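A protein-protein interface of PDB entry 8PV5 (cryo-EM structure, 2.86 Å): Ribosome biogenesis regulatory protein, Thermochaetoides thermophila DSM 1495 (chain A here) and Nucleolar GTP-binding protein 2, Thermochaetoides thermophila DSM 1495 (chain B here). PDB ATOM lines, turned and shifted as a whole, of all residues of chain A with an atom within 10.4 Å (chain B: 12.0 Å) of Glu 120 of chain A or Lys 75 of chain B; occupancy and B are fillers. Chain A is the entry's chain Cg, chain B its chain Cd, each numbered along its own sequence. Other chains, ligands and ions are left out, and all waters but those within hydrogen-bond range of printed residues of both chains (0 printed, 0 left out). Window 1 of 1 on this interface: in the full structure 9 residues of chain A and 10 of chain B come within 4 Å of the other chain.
NH1 of Arg 123 of chain A is in salt-bridge range of OE2 of Glu 71 of chain B, at 2.7 Å.
The side-chain amide nitrogen (ND2) of Asn 73 of chain B lies close to the guanidinium group (NH1) of Arg 123 of chain A (3.4 Å).
The side-chain amino group of Lys 75 of chain B lies within salt-bridge range of the side-chain carboxylate of Glu 120 of chain A (3.1 Å).
ND2 of Asn 73 of chain B is in hydrogen-bond range of OE2 of Glu 71 of chain B.
O of Glu 71 of chain B lies within hydrogen-bond range of NE1 of Trp 76 of chain B (3.1 Å).
The backbone NH (N) of Lys 75 of chain B lies close to the side-chain amide oxygen (OD1) of Asn 73 of chain B (3.3 Å).
OG1 of Thr 78 of chain B sits at hydrogen-bond distance from O of Lys 75 of chain B (3.3 Å).
O of Arg 123 of chain A is in hydrogen-bond range of NZ of Lys 137 of chain A (3.2 Å).
Among the printed residues, merely in contact across the chains: Leu 125 of chain A with Glu 71 of chain B (3.8 Å), Trp 134 of chain A with Val 69 of chain B (3.5 Å), Trp 134 of chain A with Ile 70 of chain B (3.8 Å) and Trp 134 of chain A with Glu 71 of chain B (3.5 Å).
Glu 120 of chain A touches just one residue of chain B: Lys 75.
Printed residues of chain A within 4 Å of Lys 75 of chain B: Glu 120 (3.1 Å).
No residue of chain B comes within 4 Å of Thr 118 of chain A.
Arg 123 of chain A touches two residues of chain B.
Of chain A, only Arg 123 (3.4 Å) comes within 4 Å of Asn 73 of chain B.
No residue of chain A comes within 4 Å of Arg 74 of chain B.
No residue of chain A comes within 4 Å of Trp 76 of chain B.
No residue of chain A comes within 4 Å of Thr 78 of chain B.
Of the printed residues of chain A, Glu 71 of chain B touches Arg 123, Leu 125 and Trp 134.
Printed residues of chain A within 4 Å of Ile 70 of chain B: Trp 134 (3.8 Å).
Printed residues of chain A within 4 Å of Val 69 of chain B: Trp 134.
Lys 137 of chain A touches none of the printed residues of chain B.
The nearest residue of chain B that does not touch Glu 120 of chain A is Glu 71 of chain B (5.4 Å).
The nearest residue of chain A that does not touch Lys 75 of chain B is Arg 123 of chain A (4.9 Å).
The nearest printed residue of chain B that does not touch Leu 125 of chain A is Pro 72 of chain B (5.5 Å).
Hydrophobic or aromatic side chains of chain B within 4 Å of the printed part of chain A: Val 69.
Printed residues of chain A that touch a printed residue of chain B: Glu 120, Arg 123, Leu 125 and Trp 134.
Among the printed residues, 7 pairs touch across the chains.
Among the printed residues, Asp or Glu carboxylates within 4 Å of a Lys or Arg side-chain nitrogen of the other chain: Glu 120 of chain A with Lys 75 of chain B (3.1 Å) and Arg 123 of chain A with Glu 71 of chain B (2.7 Å).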
ATOM      1  N   PRO A 116     -10.738  -1.368 -41.518  1.00  0.00           N
ATOM      2  CA  PRO A 116     -10.874  -1.805 -40.123  1.00  0.00           C
ATOM      3  C   PRO A 116     -10.578  -0.667 -39.158  1.00  0.00           C
ATOM      4  O   PRO A 116      -9.705   0.168 -39.404  1.00  0.00           O
ATOM      5  CB  PRO A 116      -9.844  -2.935 -40.002  1.00  0.00           C
ATOM      6  CG  PRO A 116      -8.886  -2.703 -41.120  1.00  0.00           C
ATOM      7  CD  PRO A 116      -9.689  -2.115 -42.231  1.00  0.00           C
ATOM      8  N   LYS A 117     -11.322  -0.638 -38.056  1.00  0.00           N
ATOM      9  CA  LYS A 117     -11.144   0.408 -37.060  1.00  0.00           C
ATOM     10  C   LYS A 117      -9.823   0.226 -36.324  1.00  0.00           C
ATOM     11  O   LYS A 117      -9.343  -0.893 -36.130  1.00  0.00           O
ATOM     12  CB  LYS A 117     -12.303   0.398 -36.064  1.00  0.00           C
ATOM     13  CG  LYS A 117     -13.622   0.874 -36.641  1.00  0.00           C
ATOM     14  CD  LYS A 117     -14.803   0.278 -35.895  1.00  0.00           C
ATOM     15  CE  LYS A 117     -14.725   0.562 -34.407  1.00  0.00           C
ATOM     16  NZ  LYS A 117     -15.742  -0.213 -33.646  1.00  0.00           N
ATOM     17  N   THR A 118      -9.230   1.345 -35.921  1.00  0.00           N
ATOM     18  CA  THR A 118      -7.982   1.284 -35.178  1.00  0.00           C
ATOM     19  C   THR A 118      -8.245   0.885 -33.731  1.00  0.00           C
ATOM     20  O   THR A 118      -9.360   1.018 -33.215  1.00  0.00           O
ATOM     21  CB  THR A 118      -7.248   2.624 -35.234  1.00  0.00           C
ATOM     22  OG1 THR A 118      -7.973   3.606 -34.488  1.00  0.00           O
ATOM     23  CG2 THR A 118      -7.110   3.094 -36.669  1.00  0.00           C
ATOM     24  N   ARG A 119      -7.194   0.373 -33.083  1.00  0.00           N
ATOM     25  CA  ARG A 119      -7.309  -0.077 -31.701  1.00  0.00           C
ATOM     26  C   ARG A 119      -7.605   1.080 -30.760  1.00  0.00           C
ATOM     27  O   ARG A 119      -8.312   0.900 -29.762  1.00  0.00           O
ATOM     28  CB  ARG A 119      -6.030  -0.793 -31.274  1.00  0.00           C
ATOM     29  CG  ARG A 119      -5.673  -1.984 -32.141  1.00  0.00           C
ATOM     30  CD  ARG A 119      -4.426  -2.677 -31.634  1.00  0.00           C
ATOM     31  NE  ARG A 119      -4.674  -3.388 -30.387  1.00  0.00           N
ATOM     32  CZ  ARG A 119      -4.987  -4.674 -30.308  1.00  0.00           C
ATOM     33  NH1 ARG A 119      -5.090  -5.428 -31.389  1.00  0.00           N
ATOM     34  NH2 ARG A 119      -5.200  -5.216 -29.114  1.00  0.00           N
ATOM     35  N   GLU A 120      -7.077   2.268 -31.058  1.00  0.00           N
ATOM     36  CA  GLU A 120      -7.393   3.444 -30.255  1.00  0.00           C
ATOM     37  C   GLU A 120      -8.844   3.863 -30.449  1.00  0.00           C
ATOM     38  O   GLU A 120      -9.488   4.346 -29.511  1.00  0.00           O
ATOM     39  CB  GLU A 120      -6.449   4.590 -30.615  1.00  0.00           C
ATOM     40  CG  GLU A 120      -4.992   4.336 -30.255  1.00  0.00           C
ATOM     41  CD  GLU A 120      -4.754   4.259 -28.759  1.00  0.00           C
ATOM     42  OE1 GLU A 120      -5.469   4.946 -27.999  1.00  0.00           O
ATOM     43  OE2 GLU A 120      -3.846   3.509 -28.343  1.00  0.00           O
ATOM     44  N   GLN A 121      -9.372   3.688 -31.662  1.00  0.00           N
ATOM     45  CA  GLN A 121     -10.759   4.043 -31.939  1.00  0.00           C
ATOM     46  C   GLN A 121     -11.744   3.069 -31.312  1.00  0.00           C
ATOM     47  O   GLN A 121     -12.839   3.483 -30.914  1.00  0.00           O
ATOM     48  CB  GLN A 121     -10.988   4.107 -33.448  1.00  0.00           C
ATOM     49  CG  GLN A 121     -12.224   4.867 -33.871  1.00  0.00           C
ATOM     50  CD  GLN A 121     -12.669   4.504 -35.272  1.00  0.00           C
ATOM     51  OE1 GLN A 121     -13.783   4.025 -35.477  1.00  0.00           O
ATOM     52  NE2 GLN A 121     -11.793   4.722 -36.245  1.00  0.00           N
ATOM     53  N   ARG A 122     -11.391   1.789 -31.214  1.00  0.00           N
ATOM     54  CA  ARG A 122     -12.307   0.776 -30.710  1.00  0.00           C
ATOM     55  C   ARG A 122     -12.166   0.532 -29.210  1.00  0.00           C
ATOM     56  O   ARG A 122     -12.672  -0.478 -28.707  1.00  0.00           O
ATOM     57  CB  ARG A 122     -12.118  -0.531 -31.482  1.00  0.00           C
ATOM     58  CG  ARG A 122     -10.807  -1.235 -31.211  1.00  0.00           C
ATOM     59  CD  ARG A 122     -10.452  -2.174 -32.339  1.00  0.00           C
ATOM     60  NE  ARG A 122      -9.477  -3.170 -31.917  1.00  0.00           N
ATOM     61  CZ  ARG A 122      -8.892  -4.033 -32.733  1.00  0.00           C
ATOM     62  NH1 ARG A 122      -9.146  -4.038 -34.029  1.00  0.00           N
ATOM     63  NH2 ARG A 122      -8.029  -4.913 -32.234  1.00  0.00           N
ATOM     64  N   ARG A 123     -11.508   1.434 -28.484  1.00  0.00           N
ATOM     65  CA  ARG A 123     -11.364   1.287 -27.041  1.00  0.00           C
ATOM     66  C   ARG A 123     -12.703   1.456 -26.335  1.00  0.00           C
ATOM     67  O   ARG A 123     -13.556   2.248 -26.746  1.00  0.00           O
ATOM     68  CB  ARG A 123     -10.365   2.305 -26.491  1.00  0.00           C
ATOM     69  CG  ARG A 123      -8.916   1.969 -26.766  1.00  0.00           C
ATOM     70  CD  ARG A 123      -7.976   2.879 -25.997  1.00  0.00           C
ATOM     71  NE  ARG A 123      -8.206   2.809 -24.559  1.00  0.00           N
ATOM     72  CZ  ARG A 123      -7.638   3.613 -23.671  1.00  0.00           C
ATOM     73  NH1 ARG A 123      -6.804   4.570 -24.040  1.00  0.00           N
ATOM     74  NH2 ARG A 123      -7.913   3.450 -22.381  1.00  0.00           N
ATOM     75  N   ASN A 124     -12.879   0.702 -25.248  1.00  0.00           N
ATOM     76  CA  ASN A 124     -14.088   0.772 -24.426  1.00  0.00           C
ATOM     77  C   ASN A 124     -13.919   1.879 -23.383  1.00  0.00           C
ATOM     78  O   ASN A 124     -13.881   1.652 -22.173  1.00  0.00           O
ATOM     79  CB  ASN A 124     -14.367  -0.575 -23.775  1.00  0.00           C
ATOM     80  CG  ASN A 124     -15.725  -0.630 -23.105  1.00  0.00           C
ATOM     81  OD1 ASN A 124     -16.572   0.234 -23.322  1.00  0.00           O
ATOM     82  ND2 ASN A 124     -15.934  -1.645 -22.276  1.00  0.00           N
ATOM     83  N   LEU A 125     -13.815   3.106 -23.884  1.00  0.00           N
ATOM     84  CA  LEU A 125     -13.633   4.261 -23.020  1.00  0.00           C
ATOM     85  C   LEU A 125     -14.091   5.508 -23.760  1.00  0.00           C
ATOM     86  O   LEU A 125     -13.782   5.684 -24.940  1.00  0.00           O
ATOM     87  CB  LEU A 125     -12.170   4.409 -22.585  1.00  0.00           C
ATOM     88  CG  LEU A 125     -11.910   5.339 -21.402  1.00  0.00           C
ATOM     89  CD1 LEU A 125     -12.684   4.882 -20.179  1.00  0.00           C
ATOM     90  CD2 LEU A 125     -10.425   5.416 -21.101  1.00  0.00           C
ATOM     91  N   GLN A 126     -14.821   6.366 -23.056  1.00  0.00           N
ATOM     92  CA  GLN A 126     -15.241   7.643 -23.610  1.00  0.00           C
ATOM     93  C   GLN A 126     -15.305   8.654 -22.479  1.00  0.00           C
ATOM     94  O   GLN A 126     -15.395   8.286 -21.305  1.00  0.00           O
ATOM     95  CB  GLN A 126     -16.597   7.543 -24.315  1.00  0.00           C
ATOM     96  CG  GLN A 126     -17.769   7.325 -23.376  1.00  0.00           C
ATOM     97  CD  GLN A 126     -19.101   7.415 -24.083  1.00  0.00           C
ATOM     98  OE1 GLN A 126     -19.174   7.344 -25.309  1.00  0.00           O
ATOM     99  NE2 GLN A 126     -20.169   7.579 -23.313  1.00  0.00           N
ATOM    100  N   TRP A 134     -14.600   9.874 -17.034  1.00  0.00           N
ATOM    101  CA  TRP A 134     -14.385   8.846 -18.041  1.00  0.00           C
ATOM    102  C   TRP A 134     -15.226   7.620 -17.718  1.00  0.00           C
ATOM    103  O   TRP A 134     -15.309   7.194 -16.562  1.00  0.00           O
ATOM    104  CB  TRP A 134     -12.908   8.467 -18.119  1.00  0.00           C
ATOM    105  CG  TRP A 134     -12.063   9.528 -18.738  1.00  0.00           C
ATOM    106  CD1 TRP A 134     -11.437  10.555 -18.098  1.00  0.00           C
ATOM    107  CD2 TRP A 134     -11.749   9.668 -20.126  1.00  0.00           C
ATOM    108  NE1 TRP A 134     -10.754  11.329 -19.004  1.00  0.00           N
ATOM    109  CE2 TRP A 134     -10.930  10.803 -20.256  1.00  0.00           C
ATOM    110  CE3 TRP A 134     -12.084   8.943 -21.273  1.00  0.00           C
ATOM    111  CZ2 TRP A 134     -10.441  11.230 -21.486  1.00  0.00           C
ATOM    112  CZ3 TRP A 134     -11.596   9.370 -22.493  1.00  0.00           C
ATOM    113  CH2 TRP A 134     -10.783  10.501 -22.590  1.00  0.00           C
ATOM    114  N   LYS A 137     -18.113   2.520 -22.735  1.00  0.00           N
ATOM    115  CA  LYS A 137     -19.230   2.513 -23.671  1.00  0.00           C
ATOM    116  C   LYS A 137     -20.133   1.304 -23.470  1.00  0.00           C
ATOM    117  O   LYS A 137     -21.354   1.414 -23.626  1.00  0.00           O
ATOM    118  CB  LYS A 137     -18.720   2.536 -25.112  1.00  0.00           C
ATOM    119  CG  LYS A 137     -17.677   3.597 -25.399  1.00  0.00           C
ATOM    120  CD  LYS A 137     -17.056   3.378 -26.768  1.00  0.00           C
ATOM    121  CE  LYS A 137     -16.124   4.513 -27.147  1.00  0.00           C
ATOM    122  NZ  LYS A 137     -15.401   4.231 -28.416  1.00  0.00           N
ATOM    123  N   VAL B  69      -9.227  16.329 -23.843  1.00  0.00           N
ATOM    124  CA  VAL B  69      -8.883  15.726 -22.562  1.00  0.00           C
ATOM    125  C   VAL B  69      -8.008  14.503 -22.804  1.00  0.00           C
ATOM    126  O   VAL B  69      -8.059  13.892 -23.876  1.00  0.00           O
ATOM    127  CB  VAL B  69     -10.144  15.347 -21.756  1.00  0.00           C
ATOM    128  CG1 VAL B  69     -10.881  16.589 -21.299  1.00  0.00           C
ATOM    129  CG2 VAL B  69     -11.066  14.515 -22.612  1.00  0.00           C
ATOM    130  N   ILE B  70      -7.199  14.155 -21.806  1.00  0.00           N
ATOM    131  CA  ILE B  70      -6.326  12.985 -21.846  1.00  0.00           C
ATOM    132  C   ILE B  70      -6.764  12.037 -20.738  1.00  0.00           C
ATOM    133  O   ILE B  70      -6.870  12.442 -19.573  1.00  0.00           O
ATOM    134  CB  ILE B  70      -4.847  13.370 -21.685  1.00  0.00           C
ATOM    135  CG1 ILE B  70      -4.411  14.337 -22.787  1.00  0.00           C
ATOM    136  CG2 ILE B  70      -3.969  12.126 -21.675  1.00  0.00           C
ATOM    137  CD1 ILE B  70      -4.213  13.686 -24.138  1.00  0.00           C
ATOM    138  N   GLU B  71      -7.021  10.780 -21.095  1.00  0.00           N
ATOM    139  CA  GLU B  71      -7.439   9.815 -20.092  1.00  0.00           C
ATOM    140  C   GLU B  71      -6.244   9.348 -19.263  1.00  0.00           C
ATOM    141  O   GLU B  71      -5.103   9.368 -19.736  1.00  0.00           O
ATOM    142  CB  GLU B  71      -8.128   8.619 -20.751  1.00  0.00           C
ATOM    143  CG  GLU B  71      -7.224   7.464 -21.169  1.00  0.00           C
ATOM    144  CD  GLU B  71      -6.543   7.694 -22.505  1.00  0.00           C
ATOM    145  OE1 GLU B  71      -6.787   8.746 -23.131  1.00  0.00           O
ATOM    146  OE2 GLU B  71      -5.766   6.816 -22.934  1.00  0.00           O
ATOM    147  N   PRO B  72      -6.470   8.969 -18.006  1.00  0.00           N
ATOM    148  CA  PRO B  72      -5.392   8.351 -17.230  1.00  0.00           C
ATOM    149  C   PRO B  72      -5.098   6.948 -17.736  1.00  0.00           C
ATOM    150  O   PRO B  72      -5.995   6.114 -17.866  1.00  0.00           O
ATOM    151  CB  PRO B  72      -5.945   8.329 -15.799  1.00  0.00           C
ATOM    152  CG  PRO B  72      -7.418   8.454 -15.952  1.00  0.00           C
ATOM    153  CD  PRO B  72      -7.643   9.281 -17.174  1.00  0.00           C
ATOM    154  N   ASN B  73      -3.825   6.698 -18.021  1.00  0.00           N
ATOM    155  CA  ASN B  73      -3.412   5.427 -18.594  1.00  0.00           C
ATOM    156  C   ASN B  73      -2.040   5.071 -18.047  1.00  0.00           C
ATOM    157  O   ASN B  73      -1.183   5.943 -17.896  1.00  0.00           O
ATOM    158  CB  ASN B  73      -3.375   5.494 -20.124  1.00  0.00           C
ATOM    159  CG  ASN B  73      -3.545   4.137 -20.774  1.00  0.00           C
ATOM    160  OD1 ASN B  73      -3.049   3.128 -20.274  1.00  0.00           O
ATOM    161  ND2 ASN B  73      -4.246   4.107 -21.899  1.00  0.00           N
ATOM    162  N   ARG B  74      -1.839   3.781 -17.766  1.00  0.00           N
ATOM    163  CA  ARG B  74      -0.551   3.330 -17.253  1.00  0.00           C
ATOM    164  C   ARG B  74       0.523   3.347 -18.333  1.00  0.00           C
ATOM    165  O   ARG B  74       1.715   3.269 -18.020  1.00  0.00           O
ATOM    166  CB  ARG B  74      -0.684   1.927 -16.660  1.00  0.00           C
ATOM    167  N   LYS B  75       0.122   3.448 -19.603  1.00  0.00           N
ATOM    168  CA  LYS B  75       1.086   3.430 -20.697  1.00  0.00           C
ATOM    169  C   LYS B  75       1.903   4.713 -20.766  1.00  0.00           C
ATOM    170  O   LYS B  75       2.973   4.732 -21.385  1.00  0.00           O
ATOM    171  CB  LYS B  75       0.360   3.192 -22.025  1.00  0.00           C
ATOM    172  CG  LYS B  75      -0.417   4.397 -22.531  1.00  0.00           C
ATOM    173  CD  LYS B  75      -0.748   4.291 -24.009  1.00  0.00           C
ATOM    174  CE  LYS B  75      -1.829   3.259 -24.262  1.00  0.00           C
ATOM    175  NZ  LYS B  75      -2.311   3.300 -25.668  1.00  0.00           N
ATOM    176  N   TRP B  76       1.427   5.794 -20.141  1.00  0.00           N
ATOM    177  CA  TRP B  76       2.129   7.068 -20.229  1.00  0.00           C
ATOM    178  C   TRP B  76       3.404   7.099 -19.400  1.00  0.00           C
ATOM    179  O   TRP B  76       4.280   7.926 -19.668  1.00  0.00           O
ATOM    180  CB  TRP B  76       1.224   8.220 -19.786  1.00  0.00           C
ATOM    181  CG  TRP B  76      -0.113   8.345 -20.482  1.00  0.00           C
ATOM    182  CD1 TRP B  76      -1.319   8.545 -19.878  1.00  0.00           C
ATOM    183  CD2 TRP B  76      -0.376   8.329 -21.897  1.00  0.00           C
ATOM    184  NE1 TRP B  76      -2.314   8.633 -20.816  1.00  0.00           N
ATOM    185  CE2 TRP B  76      -1.764   8.504 -22.062  1.00  0.00           C
ATOM    186  CE3 TRP B  76       0.422   8.176 -23.037  1.00  0.00           C
ATOM    187  CZ2 TRP B  76      -2.368   8.528 -23.315  1.00  0.00           C
ATOM    188  CZ3 TRP B  76      -0.182   8.197 -24.276  1.00  0.00           C
ATOM    189  CH2 TRP B  76      -1.562   8.373 -24.407  1.00  0.00           C
ATOM    190  N   PHE B  77       3.529   6.225 -18.402  1.00  0.00           N
ATOM    191  CA  PHE B  77       4.629   6.287 -17.450  1.00  0.00           C
ATOM    192  C   PHE B  77       5.602   5.125 -17.607  1.00  0.00           C
ATOM    193  O   PHE B  77       6.416   4.878 -16.712  1.00  0.00           O
ATOM    194  CB  PHE B  77       4.081   6.345 -16.025  1.00  0.00           C
ATOM    195  CG  PHE B  77       3.195   7.531 -15.770  1.00  0.00           C
ATOM    196  CD1 PHE B  77       1.825   7.441 -15.945  1.00  0.00           C
ATOM    197  CD2 PHE B  77       3.735   8.740 -15.371  1.00  0.00           C
ATOM    198  CE1 PHE B  77       1.012   8.532 -15.722  1.00  0.00           C
ATOM    199  CE2 PHE B  77       2.925   9.834 -15.144  1.00  0.00           C
ATOM    200  CZ  PHE B  77       1.562   9.729 -15.320  1.00  0.00           C
ATOM    201  N   THR B  78       5.540   4.414 -18.726  1.00  0.00           N
ATOM    202  CA  THR B  78       6.449   3.318 -19.019  1.00  0.00           C
ATOM    203  C   THR B  78       7.380   3.702 -20.162  1.00  0.00           C
ATOM    204  O   THR B  78       7.158   4.677 -20.883  1.00  0.00           O
ATOM    205  CB  THR B  78       5.676   2.043 -19.372  1.00  0.00           C
ATOM    206  OG1 THR B  78       5.029   2.209 -20.639  1.00  0.00           O
ATOM    207  CG2 THR B  78       4.635   1.738 -18.309  1.00  0.00           C
ATOM    208  N   ASN B  79       8.441   2.915 -20.314  1.00  0.00           N
ATOM    209  CA  ASN B  79       9.402   3.130 -21.385  1.00  0.00           C
ATOM    210  C   ASN B  79       8.879   2.520 -22.677  1.00  0.00           C
ATOM    211  O   ASN B  79       8.602   1.319 -22.738  1.00  0.00           O
ATOM    212  CB  ASN B  79      10.750   2.513 -21.020  1.00  0.00           C
ATOM    213  CG  ASN B  79      11.264   2.991 -19.682  1.00  0.00           C
ATOM    214  OD1 ASN B  79      11.284   4.188 -19.404  1.00  0.00           O
ATOM    215  ND2 ASN B  79      11.680   2.054 -18.839  1.00  0.00           N
ATOM    216  N   THR B  80       8.742   3.348 -23.711  1.00  0.00           N
ATOM    217  CA  THR B  80       8.271   2.856 -24.999  1.00  0.00           C
ATOM    218  C   THR B  80       9.341   2.060 -25.732  1.00  0.00           C
ATOM    219  O   THR B  80       9.040   1.022 -26.330  1.00  0.00           O
ATOM    220  CB  THR B  80       7.806   4.018 -25.878  1.00  0.00           C
ATOM    221  OG1 THR B  80       8.943   4.648 -26.478  1.00  0.00           O
ATOM    222  CG2 THR B  80       7.060   5.036 -25.050  1.00  0.00           C
ATOM    223  N   ARG B  81      10.588   2.522 -25.692  1.00  0.00           N
ATOM    224  CA  ARG B  81      11.682   1.867 -26.391  1.00  0.00           C
ATOM    225  C   ARG B  81      12.803   1.574 -25.410  1.00  0.00           C
ATOM    226  O   ARG B  81      13.215   2.457 -24.653  1.00  0.00           O
ATOM    227  CB  ARG B  81      12.197   2.739 -27.540  1.00  0.00           C
ATOM    228  CG  ARG B  81      11.138   3.057 -28.568  1.00  0.00           C
ATOM    229  CD  ARG B  81      11.615   4.081 -29.569  1.00  0.00           C
ATOM    230  NE  ARG B  81      10.590   4.349 -30.568  1.00  0.00           N
ATOM    231  CZ  ARG B  81      10.489   3.708 -31.723  1.00  0.00           C
ATOM    232  NH1 ARG B  81      11.350   2.764 -32.067  1.00  0.00           N
ATOM    233  NH2 ARG B  81       9.499   4.019 -32.552  1.00  0.00           N
ATOM    234  N   VAL B  82      13.282   0.334 -25.420  1.00  0.00           N
ATOM    235  CA  VAL B  82      14.420  -0.085 -24.616  1.00  0.00           C
ATOM    236  C   VAL B  82      15.402  -0.803 -25.529  1.00  0.00           C
ATOM    237  O   VAL B  82      15.025  -1.339 -26.576  1.00  0.00           O
ATOM    238  CB  VAL B  82      14.009  -0.993 -23.434  1.00  0.00           C
ATOM    239  CG1 VAL B  82      13.175  -0.219 -22.425  1.00  0.00           C
ATOM    240  CG2 VAL B  82      13.247  -2.207 -23.934  1.00  0.00           C
